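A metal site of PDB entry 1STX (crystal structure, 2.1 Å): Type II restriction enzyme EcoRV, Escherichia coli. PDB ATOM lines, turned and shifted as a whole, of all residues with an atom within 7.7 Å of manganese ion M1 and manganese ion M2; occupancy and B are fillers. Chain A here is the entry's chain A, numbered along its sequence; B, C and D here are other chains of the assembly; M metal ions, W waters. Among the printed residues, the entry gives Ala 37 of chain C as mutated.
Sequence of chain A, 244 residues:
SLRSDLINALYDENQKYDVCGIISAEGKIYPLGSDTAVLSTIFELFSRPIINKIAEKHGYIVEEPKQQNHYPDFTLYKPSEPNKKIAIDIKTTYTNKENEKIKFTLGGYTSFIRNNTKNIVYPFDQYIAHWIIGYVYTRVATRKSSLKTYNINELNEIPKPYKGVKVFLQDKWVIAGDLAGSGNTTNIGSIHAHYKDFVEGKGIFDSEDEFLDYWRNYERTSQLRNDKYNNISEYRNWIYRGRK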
ATOM      1  N   SER A  40      -5.869   4.921 -11.140  1.00  0.00           N
ATOM      2  CA  SER A  40      -6.377   5.802 -12.200  1.00  0.00           C
ATOM      3  C   SER A  40      -6.889   4.942 -13.354  1.00  0.00           C
ATOM      4  O   SER A  40      -7.807   5.329 -14.049  1.00  0.00           O
ATOM      5  CB  SER A  40      -5.331   6.784 -12.707  1.00  0.00           C
ATOM      6  OG  SER A  40      -4.272   6.079 -13.226  1.00  0.00           O
ATOM      7  N   THR A  41      -6.295   3.756 -13.552  1.00  0.00           N
ATOM      8  CA  THR A  41      -6.792   2.831 -14.578  1.00  0.00           C
ATOM      9  C   THR A  41      -8.196   2.366 -14.172  1.00  0.00           C
ATOM     10  O   THR A  41      -9.104   2.386 -14.998  1.00  0.00           O
ATOM     11  CB  THR A  41      -5.917   1.563 -14.747  1.00  0.00           C
ATOM     12  OG1 THR A  41      -4.748   1.930 -15.452  1.00  0.00           O
ATOM     13  CG2 THR A  41      -6.630   0.475 -15.589  1.00  0.00           C
ATOM     14  N   GLU A  44     -11.008   5.151 -14.523  1.00  0.00           N
ATOM     15  CA  GLU A  44     -11.282   5.493 -15.888  1.00  0.00           C
ATOM     16  C   GLU A  44     -12.209   4.437 -16.519  1.00  0.00           C
ATOM     17  O   GLU A  44     -13.218   4.785 -17.156  1.00  0.00           O
ATOM     18  CB  GLU A  44      -9.956   5.629 -16.670  1.00  0.00           C
ATOM     19  CG  GLU A  44      -9.241   6.997 -16.412  1.00  0.00           C
ATOM     20  CD  GLU A  44      -8.378   7.537 -17.623  1.00  0.00           C
ATOM     21  OE1 GLU A  44      -8.536   6.979 -18.753  1.00  0.00           O
ATOM     22  OE2 GLU A  44      -7.558   8.510 -17.414  1.00  0.00           O
ATOM     23  N   GLU A  64     -13.709   7.339 -28.164  1.00  0.00           N
ATOM     24  CA  GLU A  64     -12.471   7.265 -27.370  1.00  0.00           C
ATOM     25  C   GLU A  64     -11.317   7.356 -28.356  1.00  0.00           C
ATOM     26  O   GLU A  64     -11.506   7.172 -29.548  1.00  0.00           O
ATOM     27  CB  GLU A  64     -12.409   5.966 -26.591  1.00  0.00           C
ATOM     28  CG  GLU A  64     -13.487   5.839 -25.561  1.00  0.00           C
ATOM     29  CD  GLU A  64     -13.397   4.513 -24.823  1.00  0.00           C
ATOM     30  OE1 GLU A  64     -14.145   3.607 -25.245  1.00  0.00           O
ATOM     31  OE2 GLU A  64     -12.574   4.397 -23.852  1.00  0.00           O
ATOM     32  N   PRO A  65     -10.125   7.645 -27.895  1.00  0.00           N
ATOM     33  CA  PRO A  65      -9.067   7.718 -28.905  1.00  0.00           C
ATOM     34  C   PRO A  65      -8.776   6.370 -29.609  1.00  0.00           C
ATOM     35  O   PRO A  65      -8.881   5.278 -29.003  1.00  0.00           O
ATOM     36  CB  PRO A  65      -7.863   8.235 -28.117  1.00  0.00           C
ATOM     37  CG  PRO A  65      -8.512   8.971 -26.939  1.00  0.00           C
ATOM     38  CD  PRO A  65      -9.632   8.076 -26.574  1.00  0.00           C
ATOM     39  N   HIS A  70      -3.154  10.118 -27.166  1.00  0.00           N
ATOM     40  CA  HIS A  70      -3.970  11.144 -27.689  1.00  0.00           C
ATOM     41  C   HIS A  70      -5.033  11.558 -26.697  1.00  0.00           C
ATOM     42  O   HIS A  70      -5.708  10.743 -26.081  1.00  0.00           O
ATOM     43  CB  HIS A  70      -4.632  10.703 -28.984  1.00  0.00           C
ATOM     44  CG  HIS A  70      -3.738  10.816 -30.158  1.00  0.00           C
ATOM     45  ND1 HIS A  70      -2.612  10.044 -30.301  1.00  0.00           N
ATOM     46  CD2 HIS A  70      -3.717  11.707 -31.175  1.00  0.00           C
ATOM     47  CE1 HIS A  70      -1.935  10.458 -31.347  1.00  0.00           C
ATOM     48  NE2 HIS A  70      -2.578  11.479 -31.906  1.00  0.00           N
ATOM     49  N   TYR A  71      -5.172  12.869 -26.520  1.00  0.00           N
ATOM     50  CA  TYR A  71      -6.214  13.409 -25.658  1.00  0.00           C
ATOM     51  C   TYR A  71      -7.485  13.559 -26.578  1.00  0.00           C
ATOM     52  O   TYR A  71      -7.363  13.688 -27.813  1.00  0.00           O
ATOM     53  CB  TYR A  71      -5.737  14.757 -25.108  1.00  0.00           C
ATOM     54  CG  TYR A  71      -6.814  15.676 -24.582  1.00  0.00           C
ATOM     55  CD1 TYR A  71      -7.529  16.544 -25.457  1.00  0.00           C
ATOM     56  CD2 TYR A  71      -7.058  15.770 -23.203  1.00  0.00           C
ATOM     57  CE1 TYR A  71      -8.463  17.489 -24.956  1.00  0.00           C
ATOM     58  CE2 TYR A  71      -8.007  16.706 -22.678  1.00  0.00           C
ATOM     59  CZ  TYR A  71      -8.698  17.557 -23.565  1.00  0.00           C
ATOM     60  OH  TYR A  71      -9.566  18.470 -23.028  1.00  0.00           O
ATOM     61  N   PRO A  72      -8.701  13.507 -25.985  1.00  0.00           N
ATOM     62  CA  PRO A  72      -9.040  13.310 -24.567  1.00  0.00           C
ATOM     63  C   PRO A  72      -9.625  11.899 -24.432  1.00  0.00           C
ATOM     64  O   PRO A  72      -9.907  11.260 -25.454  1.00  0.00           O
ATOM     65  CB  PRO A  72     -10.136  14.346 -24.328  1.00  0.00           C
ATOM     66  CG  PRO A  72     -10.968  14.226 -25.657  1.00  0.00           C
ATOM     67  CD  PRO A  72      -9.860  13.973 -26.767  1.00  0.00           C
ATOM     68  N   ASP A  73      -9.868  11.477 -23.185  1.00  0.00           N
ATOM     69  CA  ASP A  73     -10.412  10.137 -22.932  1.00  0.00           C
ATOM     70  C   ASP A  73     -11.695   9.872 -23.708  1.00  0.00           C
ATOM     71  O   ASP A  73     -11.874   8.757 -24.270  1.00  0.00           O
ATOM     72  CB  ASP A  73     -10.634   9.910 -21.436  1.00  0.00           C
ATOM     73  CG  ASP A  73      -9.314   9.649 -20.673  1.00  0.00           C
ATOM     74  OD1 ASP A  73      -8.373   9.106 -21.275  1.00  0.00           O
ATOM     75  OD2 ASP A  73      -9.262  10.012 -19.482  1.00  0.00           O
ATOM     76  N   PHE A  74     -12.547  10.899 -23.768  1.00  0.00           N
ATOM     77  CA  PHE A  74     -13.811  10.864 -24.474  1.00  0.00           C
ATOM     78  C   PHE A  74     -14.072  12.129 -25.260  1.00  0.00           C
ATOM     79  O   PHE A  74     -13.786  13.234 -24.775  1.00  0.00           O
ATOM     80  CB  PHE A  74     -14.975  10.699 -23.478  1.00  0.00           C
ATOM     81  CG  PHE A  74     -14.895   9.430 -22.725  1.00  0.00           C
ATOM     82  CD1 PHE A  74     -15.511   8.251 -23.214  1.00  0.00           C
ATOM     83  CD2 PHE A  74     -14.084   9.332 -21.590  1.00  0.00           C
ATOM     84  CE1 PHE A  74     -15.272   6.988 -22.597  1.00  0.00           C
ATOM     85  CE2 PHE A  74     -13.846   8.069 -20.974  1.00  0.00           C
ATOM     86  CZ  PHE A  74     -14.448   6.914 -21.478  1.00  0.00           C
ATOM     87  N   ILE A  88     -13.832  15.159 -22.538  1.00  0.00           N
ATOM     88  CA  ILE A  88     -13.970  14.759 -21.166  1.00  0.00           C
ATOM     89  C   ILE A  88     -12.735  13.920 -20.859  1.00  0.00           C
ATOM     90  O   ILE A  88     -12.459  12.924 -21.522  1.00  0.00           O
ATOM     91  CB  ILE A  88     -15.214  13.947 -20.935  1.00  0.00           C
ATOM     92  CG1 ILE A  88     -16.459  14.744 -21.357  1.00  0.00           C
ATOM     93  CG2 ILE A  88     -15.279  13.579 -19.486  1.00  0.00           C
ATOM     94  CD1 ILE A  88     -17.843  14.011 -20.982  1.00  0.00           C
ATOM     95  N   ASP A  89     -11.966  14.360 -19.886  1.00  0.00           N
ATOM     96  CA  ASP A  89     -10.724  13.664 -19.557  1.00  0.00           C
ATOM     97  C   ASP A  89     -10.720  13.251 -18.062  1.00  0.00           C
ATOM     98  O   ASP A  89     -10.979  14.080 -17.187  1.00  0.00           O
ATOM     99  CB  ASP A  89      -9.556  14.596 -19.893  1.00  0.00           C
ATOM    100  CG  ASP A  89      -8.284  13.830 -20.201  1.00  0.00           C
ATOM    101  OD1 ASP A  89      -7.182  14.449 -20.072  1.00  0.00           O
ATOM    102  OD2 ASP A  89      -8.356  12.640 -20.586  1.00  0.00           O
ATOM    103  N   ILE A  90     -10.434  11.971 -17.786  1.00  0.00           N
ATOM    104  CA  ILE A  90     -10.425  11.521 -16.399  1.00  0.00           C
ATOM    105  C   ILE A  90      -9.073  11.622 -15.694  1.00  0.00           C
ATOM    106  O   ILE A  90      -8.045  11.289 -16.233  1.00  0.00           O
ATOM    107  CB  ILE A  90     -11.030  10.097 -16.269  1.00  0.00           C
ATOM    108  CG1 ILE A  90     -12.452  10.095 -16.823  1.00  0.00           C
ATOM    109  CG2 ILE A  90     -11.129   9.726 -14.764  1.00  0.00           C
ATOM    110  CD1 ILE A  90     -12.793   8.832 -17.536  1.00  0.00           C
ATOM    111  N   LYS A  91      -9.048  12.148 -14.479  1.00  0.00           N
ATOM    112  CA  LYS A  91      -7.799  12.311 -13.777  1.00  0.00           C
ATOM    113  C   LYS A  91      -8.011  11.803 -12.340  1.00  0.00           C
ATOM    114  O   LYS A  91      -9.115  11.804 -11.791  1.00  0.00           O
ATOM    115  CB  LYS A  91      -7.372  13.795 -13.796  1.00  0.00           C
ATOM    116  CG  LYS A  91      -7.256  14.449 -15.206  1.00  0.00           C
ATOM    117  CD  LYS A  91      -6.028  13.941 -15.885  1.00  0.00           C
ATOM    118  CE  LYS A  91      -5.673  14.667 -17.227  1.00  0.00           C
ATOM    119  NZ  LYS A  91      -4.470  14.010 -17.782  1.00  0.00           N
ATOM    120  N   THR A  92      -6.938  11.336 -11.750  1.00  0.00           N
ATOM    121  CA  THR A  92      -6.994  10.753 -10.449  1.00  0.00           C
ATOM    122  C   THR A  92      -5.881  11.246  -9.583  1.00  0.00           C
ATOM    123  O   THR A  92      -4.832  11.587 -10.075  1.00  0.00           O
ATOM    124  CB  THR A  92      -6.906   9.242 -10.594  1.00  0.00           C
ATOM    125  OG1 THR A  92      -8.108   8.825 -11.242  1.00  0.00           O
ATOM    126  CG2 THR A  92      -6.821   8.580  -9.264  1.00  0.00           C
ATOM    127  N   ILE A 133     -13.053  14.936 -15.377  1.00  0.00           N
ATOM    128  CA  ILE A 133     -13.766  14.109 -14.357  1.00  0.00           C
ATOM    129  C   ILE A 133     -12.637  13.729 -13.419  1.00  0.00           C
ATOM    130  O   ILE A 133     -11.710  13.005 -13.793  1.00  0.00           O
ATOM    131  CB  ILE A 133     -14.482  12.816 -14.940  1.00  0.00           C
ATOM    132  CG1 ILE A 133     -15.799  13.191 -15.656  1.00  0.00           C
ATOM    133  CG2 ILE A 133     -14.859  11.903 -13.765  1.00  0.00           C
ATOM    134  CD1 ILE A 133     -16.511  12.026 -16.469  1.00  0.00           C
ATOM    135  OP3  DA B   1      -5.296   8.846 -20.364  1.00  0.00           O
ATOM    136  P    DA B   1      -4.709  10.042 -19.597  1.00  0.00           P
ATOM    137  OP1  DA B   1      -5.361  10.490 -18.273  1.00  0.00           O
ATOM    138  OP2  DA B   1      -4.444  11.286 -20.429  1.00  0.00           O
ATOM    139  O5'  DA B   1      -3.279   9.412 -19.202  1.00  0.00           O
ATOM    140  C5'  DA B   1      -3.187   8.236 -18.422  1.00  0.00           C
ATOM    141  C4'  DA B   1      -2.518   8.555 -17.124  1.00  0.00           C
ATOM    142  O4'  DA B   1      -1.068   8.628 -17.285  1.00  0.00           O
ATOM    143  C3'  DA B   1      -2.924   9.897 -16.494  1.00  0.00           C
ATOM    144  O3'  DA B   1      -3.263   9.667 -15.123  1.00  0.00           O
ATOM    145  C2'  DA B   1      -1.645  10.726 -16.549  1.00  0.00           C
ATOM    146  C1'  DA B   1      -0.630   9.630 -16.403  1.00  0.00           C
ATOM    147  N9   DA B   1       0.752   9.951 -16.706  1.00  0.00           N
ATOM    148  C8   DA B   1       1.263  10.977 -17.476  1.00  0.00           C
ATOM    149  N7   DA B   1       2.560  11.032 -17.481  1.00  0.00           N
ATOM    150  C5   DA B   1       2.940   9.958 -16.694  1.00  0.00           C
ATOM    151  C6   DA B   1       4.164   9.494 -16.329  1.00  0.00           C
ATOM    152  N6   DA B   1       5.284  10.087 -16.719  1.00  0.00           N
ATOM    153  N1   DA B   1       4.217   8.405 -15.533  1.00  0.00           N
ATOM    154  C2   DA B   1       3.077   7.836 -15.143  1.00  0.00           C
ATOM    155  N3   DA B   1       1.834   8.185 -15.430  1.00  0.00           N
ATOM    156  C4   DA B   1       1.840   9.274 -16.225  1.00  0.00           C
ATOM    157  P    DT B   2      -3.742  10.877 -14.201  1.00  0.00           P
ATOM    158  OP1  DT B   2      -5.046  10.372 -13.693  1.00  0.00           O
ATOM    159  OP2  DT B   2      -3.656  12.247 -14.838  1.00  0.00           O
ATOM    160  O5'  DT B   2      -2.611  10.914 -13.080  1.00  0.00           O
ATOM    161  C5'  DT B   2      -2.357   9.756 -12.315  1.00  0.00           C
ATOM    162  C4'  DT B   2      -1.115   9.970 -11.506  1.00  0.00           C
ATOM    163  O4'  DT B   2       0.044  10.131 -12.368  1.00  0.00           O
ATOM    164  C3'  DT B   2      -1.147  11.200 -10.612  1.00  0.00           C
ATOM    165  O3'  DT B   2      -0.465  10.779  -9.460  1.00  0.00           O
ATOM    166  C2'  DT B   2      -0.214  12.157 -11.334  1.00  0.00           C
ATOM    167  C1'  DT B   2       0.824  11.172 -11.836  1.00  0.00           C
ATOM    168  N1   DT B   2       1.802  11.627 -12.839  1.00  0.00           N
ATOM    169  C2   DT B   2       3.123  11.245 -12.652  1.00  0.00           C
ATOM    170  O2   DT B   2       3.471  10.437 -11.821  1.00  0.00           O
ATOM    171  N3   DT B   2       4.034  11.842 -13.510  1.00  0.00           N
ATOM    172  C4   DT B   2       3.744  12.749 -14.555  1.00  0.00           C
ATOM    173  O4   DT B   2       4.669  13.250 -15.210  1.00  0.00           O
ATOM    174  C5   DT B   2       2.315  13.032 -14.735  1.00  0.00           C
ATOM    175  C7   DT B   2       1.893  13.944 -15.852  1.00  0.00           C
ATOM    176  C6   DT B   2       1.439  12.457 -13.894  1.00  0.00           C
ATOM    177  N   ASP C  35      -5.840   0.277 -24.691  1.00  0.00           N
ATOM    178  CA  ASP C  35      -4.472   0.781 -24.618  1.00  0.00           C
ATOM    179  C   ASP C  35      -3.566   0.069 -23.586  1.00  0.00           C
ATOM    180  O   ASP C  35      -4.040  -0.682 -22.702  1.00  0.00           O
ATOM    181  CB  ASP C  35      -4.487   2.307 -24.414  1.00  0.00           C
ATOM    182  CG  ASP C  35      -5.391   2.730 -23.263  1.00  0.00           C
ATOM    183  OD1 ASP C  35      -6.480   2.102 -23.118  1.00  0.00           O
ATOM    184  OD2 ASP C  35      -5.027   3.707 -22.539  1.00  0.00           O
ATOM    185  N   ALA C  37      -1.903   1.433 -21.289  1.00  0.00           N
ATOM    186  CA  ALA C  37      -2.057   2.076 -19.980  1.00  0.00           C
ATOM    187  C   ALA C  37      -2.901   1.082 -19.175  1.00  0.00           C
ATOM    188  O   ALA C  37      -2.533   0.695 -18.093  1.00  0.00           O
ATOM    189  CB  ALA C  37      -2.770   3.435 -20.151  1.00  0.00           C
ATOM    190  N   VAL C  38      -4.023   0.655 -19.752  1.00  0.00           N
ATOM    191  CA  VAL C  38      -4.936  -0.315 -19.143  1.00  0.00           C
ATOM    192  C   VAL C  38      -4.383  -1.738 -19.001  1.00  0.00           C
ATOM    193  O   VAL C  38      -4.378  -2.310 -17.925  1.00  0.00           O
ATOM    194  CB  VAL C  38      -6.204  -0.435 -19.980  1.00  0.00           C
ATOM    195  CG1 VAL C  38      -7.053  -1.595 -19.470  1.00  0.00           C
ATOM    196  CG2 VAL C  38      -6.964   0.858 -19.923  1.00  0.00           C
ATOM    197  P    DT D   6       0.262  15.155 -23.882  1.00  0.00           P
ATOM    198  OP1  DT D   6      -0.877  15.975 -24.343  1.00  0.00           O
ATOM    199  OP2  DT D   6       0.965  15.493 -22.622  1.00  0.00           O
ATOM    200  O5'  DT D   6      -0.193  13.637 -23.652  1.00  0.00           O
ATOM    201  C5'  DT D   6      -1.120  13.007 -24.518  1.00  0.00           C
ATOM    202  C4'  DT D   6      -1.548  11.680 -23.927  1.00  0.00           C
ATOM    203  O4'  DT D   6      -0.392  10.841 -23.731  1.00  0.00           O
ATOM    204  C3'  DT D   6      -2.265  11.757 -22.579  1.00  0.00           C
ATOM    205  O3'  DT D   6      -3.564  11.154 -22.640  1.00  0.00           O
ATOM    206  C2'  DT D   6      -1.331  11.077 -21.595  1.00  0.00           C
ATOM    207  C1'  DT D   6      -0.324  10.305 -22.414  1.00  0.00           C
ATOM    208  N1   DT D   6       1.088  10.489 -21.932  1.00  0.00           N
ATOM    209  C2   DT D   6       1.778   9.383 -21.472  1.00  0.00           C
ATOM    210  O2   DT D   6       1.275   8.267 -21.446  1.00  0.00           O
ATOM    211  N3   DT D   6       3.060   9.648 -21.031  1.00  0.00           N
ATOM    212  C4   DT D   6       3.691  10.867 -20.987  1.00  0.00           C
ATOM    213  O4   DT D   6       4.817  10.939 -20.561  1.00  0.00           O
ATOM    214  C5   DT D   6       2.923  11.986 -21.498  1.00  0.00           C
ATOM    215  C7   DT D   6       3.533  13.368 -21.532  1.00  0.00           C
ATOM    216  C6   DT D   6       1.676  11.738 -21.926  1.00  0.00           C
HETATM  217 MN    MN M   1      -7.263  10.274 -18.404  1.00  0.00          MN
HETATM  218 MN    MN M   2      -7.015   7.552 -20.452  1.00  0.00          MN
HETATM  219  O   HOH W   1      -6.366   8.548 -22.654  1.00  0.00           O
HETATM  220  O   HOH W   2      -8.622   6.443 -21.883  1.00  0.00           O
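The nearest printed residue that does not touch manganese ion M2 is Asp 35 of chain C (4.8 Å).
Manganese ion M1 is bound by OP1 of DA 1 of chain B (1.9 Å), OE2 of Glu 44 (2.0 Å), OD2 of Asp 73 (2.3 Å) and O of Ile 90 (2.5 Å).
Manganese ion M2 is bound by OP3 of DA 1 of chain B (2.2 Å).
OD1 of Asp 73 binds manganese ion M2 (2.2 Å).
Manganese ion M2 is bound by the side-chain carboxylate (OE1) of Glu 44 (2.4 Å).
Water W2 binds manganese ion M2 (2.4 Å).
Manganese ion M2 is bound by water W1 (2.5 Å).
Manganese ion M2 has five donor atoms within binding distance.
OD2 of Asp 89 touches manganese ion M1, at 3.4 Å.
The nearest printed residue that does not touch manganese ion M1 is Lys 91 (4.6 Å).
The side-chain amino group (NZ) of Lys 91 lies within salt-bridge range of OP2 of DA 1 of chain B (3.8 Å).
OD2 of Asp 89 lies close to N of Asp 73, 3.2 Å away.
The backbone carbonyl oxygen (O) of Ile 88 sits at hydrogen-bond distance from the backbone NH (N) of Asp 73, at 3.4 Å.
The side-chain amino group (NZ) of Lys 91 lies within salt-bridge range of the side-chain carboxylate (OD1) of Asp 89, 3.6 Å away.
O of Asp 89 lies within hydrogen-bond range of N of Ile 133 (2.9 Å).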
